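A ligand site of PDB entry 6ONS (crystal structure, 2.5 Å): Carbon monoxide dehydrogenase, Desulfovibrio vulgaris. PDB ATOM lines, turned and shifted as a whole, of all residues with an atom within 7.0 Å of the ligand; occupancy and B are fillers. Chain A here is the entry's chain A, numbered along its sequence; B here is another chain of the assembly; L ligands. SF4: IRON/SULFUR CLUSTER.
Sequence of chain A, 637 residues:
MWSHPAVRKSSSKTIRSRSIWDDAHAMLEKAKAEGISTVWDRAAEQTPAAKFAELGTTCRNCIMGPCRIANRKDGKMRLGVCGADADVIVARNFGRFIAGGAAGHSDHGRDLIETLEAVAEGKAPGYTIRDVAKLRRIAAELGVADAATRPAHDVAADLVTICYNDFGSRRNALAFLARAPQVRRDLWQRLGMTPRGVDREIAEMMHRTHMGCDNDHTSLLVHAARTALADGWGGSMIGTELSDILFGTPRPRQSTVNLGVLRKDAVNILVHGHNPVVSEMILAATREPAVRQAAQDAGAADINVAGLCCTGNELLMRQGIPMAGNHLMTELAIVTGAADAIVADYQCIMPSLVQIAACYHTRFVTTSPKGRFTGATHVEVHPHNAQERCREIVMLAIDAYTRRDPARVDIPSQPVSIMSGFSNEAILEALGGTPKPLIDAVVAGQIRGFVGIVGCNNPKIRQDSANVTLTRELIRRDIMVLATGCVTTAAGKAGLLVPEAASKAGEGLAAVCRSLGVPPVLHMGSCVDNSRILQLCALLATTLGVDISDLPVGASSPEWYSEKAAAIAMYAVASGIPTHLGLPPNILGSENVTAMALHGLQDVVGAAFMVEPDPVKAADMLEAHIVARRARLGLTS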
ATOM      1  N   THR A  58      20.105 -13.961  20.286  1.00  0.00           N
ATOM      2  CA  THR A  58      18.781 -13.662  20.816  1.00  0.00           C
ATOM      3  C   THR A  58      18.204 -14.923  21.427  1.00  0.00           C
ATOM      4  O   THR A  58      18.272 -15.997  20.811  1.00  0.00           O
ATOM      5  CB  THR A  58      17.856 -13.117  19.713  1.00  0.00           C
ATOM      6  OG1 THR A  58      18.433 -11.949  19.142  1.00  0.00           O
ATOM      7  CG2 THR A  58      16.489 -12.762  20.298  1.00  0.00           C
ATOM      8  N   CYS A  59      17.654 -14.808  22.619  1.00  0.00           N
ATOM      9  CA  CYS A  59      17.125 -15.954  23.356  1.00  0.00           C
ATOM     10  C   CYS A  59      15.664 -15.713  23.702  1.00  0.00           C
ATOM     11  O   CYS A  59      15.287 -14.614  24.117  1.00  0.00           O
ATOM     12  CB  CYS A  59      17.945 -16.201  24.628  1.00  0.00           C
ATOM     13  SG  CYS A  59      17.430 -17.659  25.550  1.00  0.00           S
ATOM     14  N   ARG A  60      14.852 -16.759  23.521  1.00  0.00           N
ATOM     15  CA  ARG A  60      13.424 -16.686  23.806  1.00  0.00           C
ATOM     16  C   ARG A  60      12.966 -17.868  24.649  1.00  0.00           C
ATOM     17  O   ARG A  60      11.778 -18.212  24.646  1.00  0.00           O
ATOM     18  CB  ARG A  60      12.615 -16.632  22.500  1.00  0.00           C
ATOM     19  CG  ARG A  60      12.991 -15.468  21.585  1.00  0.00           C
ATOM     20  CD  ARG A  60      12.268 -15.561  20.248  1.00  0.00           C
ATOM     21  N   ASN A  61      13.881 -18.495  25.401  1.00  0.00           N
ATOM     22  CA  ASN A  61      13.571 -19.739  26.105  1.00  0.00           C
ATOM     23  C   ASN A  61      12.718 -19.536  27.350  1.00  0.00           C
ATOM     24  O   ASN A  61      12.277 -20.525  27.943  1.00  0.00           O
ATOM     25  CB  ASN A  61      14.859 -20.464  26.478  1.00  0.00           C
ATOM     26  CG  ASN A  61      15.642 -20.910  25.265  1.00  0.00           C
ATOM     27  OD1 ASN A  61      15.102 -21.001  24.158  1.00  0.00           O
ATOM     28  ND2 ASN A  61      16.921 -21.199  25.464  1.00  0.00           N
ATOM     29  N   CYS A  62      12.495 -18.294  27.772  1.00  0.00           N
ATOM     30  CA  CYS A  62      11.638 -18.022  28.909  1.00  0.00           C
ATOM     31  C   CYS A  62      11.143 -16.589  28.807  1.00  0.00           C
ATOM     32  O   CYS A  62      11.670 -15.776  28.036  1.00  0.00           O
ATOM     33  CB  CYS A  62      12.375 -18.259  30.240  1.00  0.00           C
ATOM     34  SG  CYS A  62      13.369 -16.870  30.819  1.00  0.00           S
ATOM     35  N   ILE A  63      10.117 -16.283  29.590  1.00  0.00           N
ATOM     36  CA  ILE A  63       9.492 -14.959  29.551  1.00  0.00           C
ATOM     37  C   ILE A  63      10.089 -14.025  30.601  1.00  0.00           C
ATOM     38  O   ILE A  63       9.491 -12.991  30.908  1.00  0.00           O
ATOM     39  CB  ILE A  63       7.961 -15.046  29.670  1.00  0.00           C
ATOM     40  CG1 ILE A  63       7.530 -15.502  31.065  1.00  0.00           C
ATOM     41  CG2 ILE A  63       7.378 -15.982  28.620  1.00  0.00           C
ATOM     42  CD1 ILE A  63       6.111 -15.105  31.435  1.00  0.00           C
ATOM     43  N   MET A  64      11.253 -14.355  31.152  1.00  0.00           N
ATOM     44  CA  MET A  64      12.056 -13.293  31.756  1.00  0.00           C
ATOM     45  C   MET A  64      12.671 -12.441  30.662  1.00  0.00           C
ATOM     46  O   MET A  64      12.914 -11.251  30.867  1.00  0.00           O
ATOM     47  CB  MET A  64      13.145 -13.850  32.667  1.00  0.00           C
ATOM     48  CG  MET A  64      12.629 -14.591  33.892  1.00  0.00           C
ATOM     49  SD  MET A  64      13.851 -14.716  35.216  1.00  0.00           S
ATOM     50  CE  MET A  64      15.257 -15.352  34.324  1.00  0.00           C
ATOM     51  N   GLY A  65      12.944 -13.050  29.503  1.00  0.00           N
ATOM     52  CA  GLY A  65      13.326 -12.320  28.321  1.00  0.00           C
ATOM     53  C   GLY A  65      12.109 -11.880  27.533  1.00  0.00           C
ATOM     54  O   GLY A  65      11.049 -11.584  28.104  1.00  0.00           O
ATOM     55  N   PRO A  66      12.212 -11.868  26.191  1.00  0.00           N
ATOM     56  CA  PRO A  66      13.365 -12.261  25.384  1.00  0.00           C
ATOM     57  C   PRO A  66      14.558 -11.307  25.516  1.00  0.00           C
ATOM     58  O   PRO A  66      14.382 -10.095  25.611  1.00  0.00           O
ATOM     59  CB  PRO A  66      12.819 -12.242  23.959  1.00  0.00           C
ATOM     60  CG  PRO A  66      11.713 -11.264  23.996  1.00  0.00           C
ATOM     61  CD  PRO A  66      11.086 -11.426  25.348  1.00  0.00           C
ATOM     62  N   CYS A  67      15.765 -11.877  25.515  1.00  0.00           N
ATOM     63  CA  CYS A  67      16.986 -11.124  25.730  1.00  0.00           C
ATOM     64  C   CYS A  67      17.799 -11.053  24.454  1.00  0.00           C
ATOM     65  O   CYS A  67      17.634 -11.864  23.527  1.00  0.00           O
ATOM     66  CB  CYS A  67      17.818 -11.759  26.855  1.00  0.00           C
ATOM     67  SG  CYS A  67      16.891 -12.078  28.374  1.00  0.00           S
ATOM     68  N   ARG A  68      18.685 -10.061  24.396  1.00  0.00           N
ATOM     69  CA  ARG A  68      19.590  -9.874  23.273  1.00  0.00           C
ATOM     70  C   ARG A  68      20.957  -9.489  23.802  1.00  0.00           C
ATOM     71  O   ARG A  68      21.061  -8.629  24.685  1.00  0.00           O
ATOM     72  CB  ARG A  68      19.069  -8.802  22.306  1.00  0.00           C
ATOM     73  N   ILE A  69      22.003 -10.123  23.272  1.00  0.00           N
ATOM     74  CA  ILE A  69      23.371  -9.864  23.681  1.00  0.00           C
ATOM     75  C   ILE A  69      24.026  -8.964  22.641  1.00  0.00           C
ATOM     76  O   ILE A  69      24.005  -9.280  21.442  1.00  0.00           O
ATOM     77  CB  ILE A  69      24.163 -11.172  23.861  1.00  0.00           C
ATOM     78  CG1 ILE A  69      23.417 -12.104  24.810  1.00  0.00           C
ATOM     79  CG2 ILE A  69      25.558 -10.881  24.386  1.00  0.00           C
ATOM     80  CD1 ILE A  69      23.182 -11.526  26.184  1.00  0.00           C
ATOM     81  N   LEU A  79      24.678  -9.651  29.229  1.00  0.00           N
ATOM     82  CA  LEU A  79      24.142 -10.896  29.734  1.00  0.00           C
ATOM     83  C   LEU A  79      22.622 -10.874  29.635  1.00  0.00           C
ATOM     84  O   LEU A  79      22.011  -9.801  29.581  1.00  0.00           O
ATOM     85  CB  LEU A  79      24.560 -11.154  31.190  1.00  0.00           C
ATOM     86  CG  LEU A  79      26.061 -11.131  31.498  1.00  0.00           C
ATOM     87  CD1 LEU A  79      26.289 -11.066  33.005  1.00  0.00           C
ATOM     88  CD2 LEU A  79      26.743 -12.352  30.914  1.00  0.00           C
ATOM     89  N   GLY A  80      22.022 -12.049  29.609  1.00  0.00           N
ATOM     90  CA  GLY A  80      20.579 -12.173  29.681  1.00  0.00           C
ATOM     91  C   GLY A  80      20.085 -11.894  31.089  1.00  0.00           C
ATOM     92  O   GLY A  80      20.845 -11.661  32.028  1.00  0.00           O
ATOM     93  N   VAL A  81      18.750 -11.928  31.240  1.00  0.00           N
ATOM     94  CA  VAL A  81      18.158 -11.682  32.551  1.00  0.00           C
ATOM     95  C   VAL A  81      18.611 -12.731  33.559  1.00  0.00           C
ATOM     96  O   VAL A  81      18.866 -12.420  34.727  1.00  0.00           O
ATOM     97  CB  VAL A  81      16.620 -11.621  32.438  1.00  0.00           C
ATOM     98  CG1 VAL A  81      15.986 -11.472  33.806  1.00  0.00           C
ATOM     99  CG2 VAL A  81      16.200 -10.472  31.530  1.00  0.00           C
ATOM    100  N   CYS A  82      18.733 -13.980  33.113  1.00  0.00           N
ATOM    101  CA  CYS A  82      19.222 -15.050  33.980  1.00  0.00           C
ATOM    102  C   CYS A  82      20.729 -15.000  34.173  1.00  0.00           C
ATOM    103  O   CYS A  82      21.250 -15.715  35.039  1.00  0.00           O
ATOM    104  CB  CYS A  82      18.827 -16.414  33.413  1.00  0.00           C
ATOM    105  SG  CYS A  82      19.526 -16.807  31.780  1.00  0.00           S
ATOM    106  N   GLY A  83      21.448 -14.193  33.402  1.00  0.00           N
ATOM    107  CA  GLY A  83      22.889 -14.130  33.487  1.00  0.00           C
ATOM    108  C   GLY A  83      23.640 -14.919  32.437  1.00  0.00           C
ATOM    109  O   GLY A  83      24.860 -15.040  32.533  1.00  0.00           O
ATOM    110  N   ALA A  84      22.943 -15.457  31.435  1.00  0.00           N
ATOM    111  CA  ALA A  84      23.612 -16.200  30.379  1.00  0.00           C
ATOM    112  C   ALA A  84      24.368 -15.241  29.461  1.00  0.00           C
ATOM    113  O   ALA A  84      23.878 -14.164  29.127  1.00  0.00           O
ATOM    114  CB  ALA A  84      22.599 -17.009  29.575  1.00  0.00           C
ATOM    115  N   ASP A  85      25.572 -15.648  29.059  1.00  0.00           N
ATOM    116  CA  ASP A  85      26.409 -14.840  28.189  1.00  0.00           C
ATOM    117  C   ASP A  85      26.162 -15.223  26.724  1.00  0.00           C
ATOM    118  O   ASP A  85      25.275 -16.023  26.418  1.00  0.00           O
ATOM    119  CB  ASP A  85      27.869 -14.980  28.588  1.00  0.00           C
ATOM    120  CG  ASP A  85      28.355 -16.413  28.582  1.00  0.00           C
ATOM    121  OD1 ASP A  85      27.592 -17.317  28.169  1.00  0.00           O
ATOM    122  OD2 ASP A  85      29.509 -16.657  29.001  1.00  0.00           O
ATOM    123  N   ILE A  89      24.020 -18.627  25.004  1.00  0.00           N
ATOM    124  CA  ILE A  89      22.823 -18.357  24.199  1.00  0.00           C
ATOM    125  C   ILE A  89      23.012 -18.889  22.782  1.00  0.00           C
ATOM    126  O   ILE A  89      22.112 -19.525  22.219  1.00  0.00           O
ATOM    127  CB  ILE A  89      22.508 -16.845  24.203  1.00  0.00           C
ATOM    128  CG1 ILE A  89      22.083 -16.410  25.606  1.00  0.00           C
ATOM    129  CG2 ILE A  89      21.438 -16.527  23.181  1.00  0.00           C
ATOM    130  CD1 ILE A  89      21.518 -15.008  25.672  1.00  0.00           C
ATOM    131  N   ARG A  92      22.922 -22.736  22.913  1.00  0.00           N
ATOM    132  CA  ARG A  92      21.595 -23.286  23.145  1.00  0.00           C
ATOM    133  C   ARG A  92      20.715 -23.171  21.910  1.00  0.00           C
ATOM    134  O   ARG A  92      19.940 -24.083  21.600  1.00  0.00           O
ATOM    135  CB  ARG A  92      20.945 -22.617  24.352  1.00  0.00           C
ATOM    136  CG  ARG A  92      21.595 -22.949  25.684  1.00  0.00           C
ATOM    137  CD  ARG A  92      20.813 -22.406  26.871  1.00  0.00           C
ATOM    138  NE  ARG A  92      20.602 -20.966  26.769  1.00  0.00           N
ATOM    139  CZ  ARG A  92      20.066 -20.221  27.739  1.00  0.00           C
ATOM    140  NH1 ARG A  92      19.704 -20.787  28.879  1.00  0.00           N
ATOM    141  NH2 ARG A  92      19.898 -18.922  27.563  1.00  0.00           N
ATOM    142  N   THR A 209      18.825 -26.989  27.151  1.00  0.00           N
ATOM    143  CA  THR A 209      18.664 -25.610  26.721  1.00  0.00           C
ATOM    144  C   THR A 209      17.569 -24.862  27.483  1.00  0.00           C
ATOM    145  O   THR A 209      17.247 -23.722  27.122  1.00  0.00           O
ATOM    146  CB  THR A 209      18.376 -25.557  25.220  1.00  0.00           C
ATOM    147  OG1 THR A 209      17.201 -26.320  24.926  1.00  0.00           O
ATOM    148  CG2 THR A 209      19.549 -26.130  24.442  1.00  0.00           C
ATOM    149  N   HIS A 210      16.981 -25.475  28.505  1.00  0.00           N
ATOM    150  CA  HIS A 210      16.093 -24.747  29.399  1.00  0.00           C
ATOM    151  C   HIS A 210      16.900 -23.803  30.279  1.00  0.00           C
ATOM    152  O   HIS A 210      18.103 -23.991  30.490  1.00  0.00           O
ATOM    153  CB  HIS A 210      15.277 -25.724  30.252  1.00  0.00           C
ATOM    154  CG  HIS A 210      14.196 -25.072  31.054  1.00  0.00           C
ATOM    155  ND1 HIS A 210      14.418 -24.516  32.304  1.00  0.00           N
ATOM    156  CD2 HIS A 210      12.878 -24.895  30.793  1.00  0.00           C
ATOM    157  CE1 HIS A 210      13.287 -24.021  32.765  1.00  0.00           C
ATOM    158  NE2 HIS A 210      12.330 -24.239  31.875  1.00  0.00           N
ATOM    159  N   MET A 211      16.229 -22.764  30.784  1.00  0.00           N
ATOM    160  CA  MET A 211      16.903 -21.800  31.658  1.00  0.00           C
ATOM    161  C   MET A 211      17.482 -22.509  32.874  1.00  0.00           C
ATOM    162  O   MET A 211      16.809 -23.327  33.508  1.00  0.00           O
ATOM    163  CB  MET A 211      15.921 -20.718  32.095  1.00  0.00           C
ATOM    164  CG  MET A 211      16.569 -19.502  32.789  1.00  0.00           C
ATOM    165  SD  MET A 211      17.240 -19.779  34.448  1.00  0.00           S
ATOM    166  CE  MET A 211      16.270 -18.638  35.429  1.00  0.00           C
ATOM    167  N   GLY A 212      18.731 -22.199  33.184  1.00  0.00           N
ATOM    168  CA  GLY A 212      19.348 -22.708  34.394  1.00  0.00           C
ATOM    169  C   GLY A 212      19.667 -24.180  34.382  1.00  0.00           C
ATOM    170  O   GLY A 212      19.697 -24.804  35.445  1.00  0.00           O
ATOM    171  N   ASN A 215      24.725 -24.526  31.118  1.00  0.00           N
ATOM    172  CA  ASN A 215      25.239 -23.187  30.862  1.00  0.00           C
ATOM    173  C   ASN A 215      26.736 -23.212  30.587  1.00  0.00           C
ATOM    174  O   ASN A 215      27.501 -22.385  31.081  1.00  0.00           O
ATOM    175  CB  ASN A 215      24.924 -22.246  32.028  1.00  0.00           C
ATOM    176  CG  ASN A 215      23.460 -21.877  32.095  1.00  0.00           C
ATOM    177  OD1 ASN A 215      23.031 -20.915  31.472  1.00  0.00           O
ATOM    178  ND2 ASN A 215      22.680 -22.654  32.841  1.00  0.00           N
ATOM    179  N   GLN B  46      17.308  -5.461  29.742  1.00  0.00           N
ATOM    180  CA  GLN B  46      16.754  -6.209  28.624  1.00  0.00           C
ATOM    181  C   GLN B  46      15.298  -5.819  28.398  1.00  0.00           C
ATOM    182  O   GLN B  46      14.493  -6.617  27.929  1.00  0.00           O
ATOM    183  CB  GLN B  46      16.849  -7.715  28.859  1.00  0.00           C
ATOM    184  CG  GLN B  46      18.264  -8.269  28.868  1.00  0.00           C
ATOM    185  CD  GLN B  46      18.872  -8.389  27.480  1.00  0.00           C
ATOM    186  OE1 GLN B  46      18.210  -8.120  26.479  1.00  0.00           O
ATOM    187  NE2 GLN B  46      20.128  -8.790  27.421  1.00  0.00           N
ATOM    188  N   PRO B 351      22.912 -18.807  35.903  1.00  0.00           N
ATOM    189  CA  PRO B 351      24.372 -18.819  35.829  1.00  0.00           C
ATOM    190  C   PRO B 351      25.025 -17.641  36.538  1.00  0.00           C
ATOM    191  O   PRO B 351      26.226 -17.701  36.824  1.00  0.00           O
ATOM    192  CB  PRO B 351      24.656 -18.794  34.317  1.00  0.00           C
ATOM    193  CG  PRO B 351      23.421 -18.214  33.711  1.00  0.00           C
ATOM    194  CD  PRO B 351      22.287 -18.682  34.569  1.00  0.00           C
ATOM    195  N   TYR B 561       7.451 -17.881  34.762  1.00  0.00           N
ATOM    196  CA  TYR B 561       8.509 -17.459  33.845  1.00  0.00           C
ATOM    197  C   TYR B 561       8.994 -18.551  32.911  1.00  0.00           C
ATOM    198  O   TYR B 561       9.377 -18.231  31.776  1.00  0.00           O
ATOM    199  CB  TYR B 561       9.719 -16.915  34.630  1.00  0.00           C
ATOM    200  CG  TYR B 561      10.843 -17.922  34.814  1.00  0.00           C
ATOM    201  CD1 TYR B 561      11.909 -17.979  33.914  1.00  0.00           C
ATOM    202  CD2 TYR B 561      10.841 -18.821  35.869  1.00  0.00           C
ATOM    203  CE1 TYR B 561      12.926 -18.900  34.071  1.00  0.00           C
ATOM    204  CE2 TYR B 561      11.851 -19.740  36.034  1.00  0.00           C
ATOM    205  CZ  TYR B 561      12.891 -19.775  35.130  1.00  0.00           C
ATOM    206  OH  TYR B 561      13.901 -20.695  35.295  1.00  0.00           O
HETATM  207 FE1  SF4 L   1      17.068 -16.775  27.618  1.00  0.00          FE
HETATM  208 FE2  SF4 L   1      16.805 -14.324  28.773  1.00  0.00          FE
HETATM  209 FE3  SF4 L   1      17.976 -16.366  30.168  1.00  0.00          FE
HETATM  210 FE4  SF4 L   1      15.297 -16.421  29.680  1.00  0.00          FE
HETATM  211  S1  SF4 L   1      16.426 -14.903  30.942  1.00  0.00           S
HETATM  212  S2  SF4 L   1      16.759 -18.151  29.418  1.00  0.00           S
HETATM  213  S3  SF4 L   1      15.208 -15.458  27.604  1.00  0.00           S
HETATM  214  S4  SF4 L   1      18.760 -15.379  28.254  1.00  0.00           S
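Residues that only touch the ligand: Asn 61 (3.98 Å), Met 64 (3.6 Å), Gly 65 (3.7 Å), Gly 80 (3.95 Å), Ile 89 (3.8 Å) and Met 211 (3.6 Å).
Hydrophobic or aromatic side chains that line the ligand: Met 64, Val 81, Ile 89 and Met 211.
12 residues have an atom within 4 Å of the ligand: Cys 59, Asn 61, Cys 62, Met 64, Gly 65, Cys 67, Gly 80, Val 81, Cys 82, Ile 89, Arg 92 and Met 211.
The nearest printed residue that does not touch the ligand is Arg 60 (4.3 Å).
The side-chain sulfur of Cys 59 binds an iron atom (FE1) of the ligand, at 2.3 Å.
The backbone NH of Cys 82 sits close to a sulfur (S1) of the ligand, at 3.3 Å.
SG of Cys 82 binds FE3 of the ligand (2.3 Å).
An iron atom (FE2) of the ligand is bound by the side-chain sulfur (SG) of Cys 67 (2.3 Å).
An iron atom (FE4) of the ligand is bound by the side-chain sulfur (SG) of Cys 62 (2.3 Å).
NH2 of Arg 92 sits close to S2 of the ligand (3.7 Å).
A sulfur (S1) of the ligand sits close to the backbone NH (N) of Val 81, at 3.8 Å.
The backbone NH (N) of Cys 59 lies within hydrogen-bond range of the backbone carbonyl oxygen (O) of Cys 67, at 3.1 Å.
The side-chain sulfur of Cys 59 lies close to the guanidinium group of Arg 92 (3.4 Å).
SG of Cys 59 sits close to ND2 of Asn 61, at 3.6 Å.
The side-chain sulfur (SG) of Cys 82 lies close to the backbone NH (N) of Ala 84 (3.7 Å).
The side-chain sulfur of Cys 67 sits close to the backbone NH of Val 81 (3.4 Å).
The backbone NH (N) of Met 64 sits close to the side-chain sulfur (SG) of Cys 62, 3.3 Å away.
The side-chain sulfur (SD) of Met 211 sits close to the side-chain hydroxyl (OH) of Tyr 561 of chain B (3.6 Å).
The backbone carbonyl oxygen (O) of Thr 209 lies within hydrogen-bond range of the side-chain amide nitrogen (ND2) of Asn 61 (3.0 Å).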
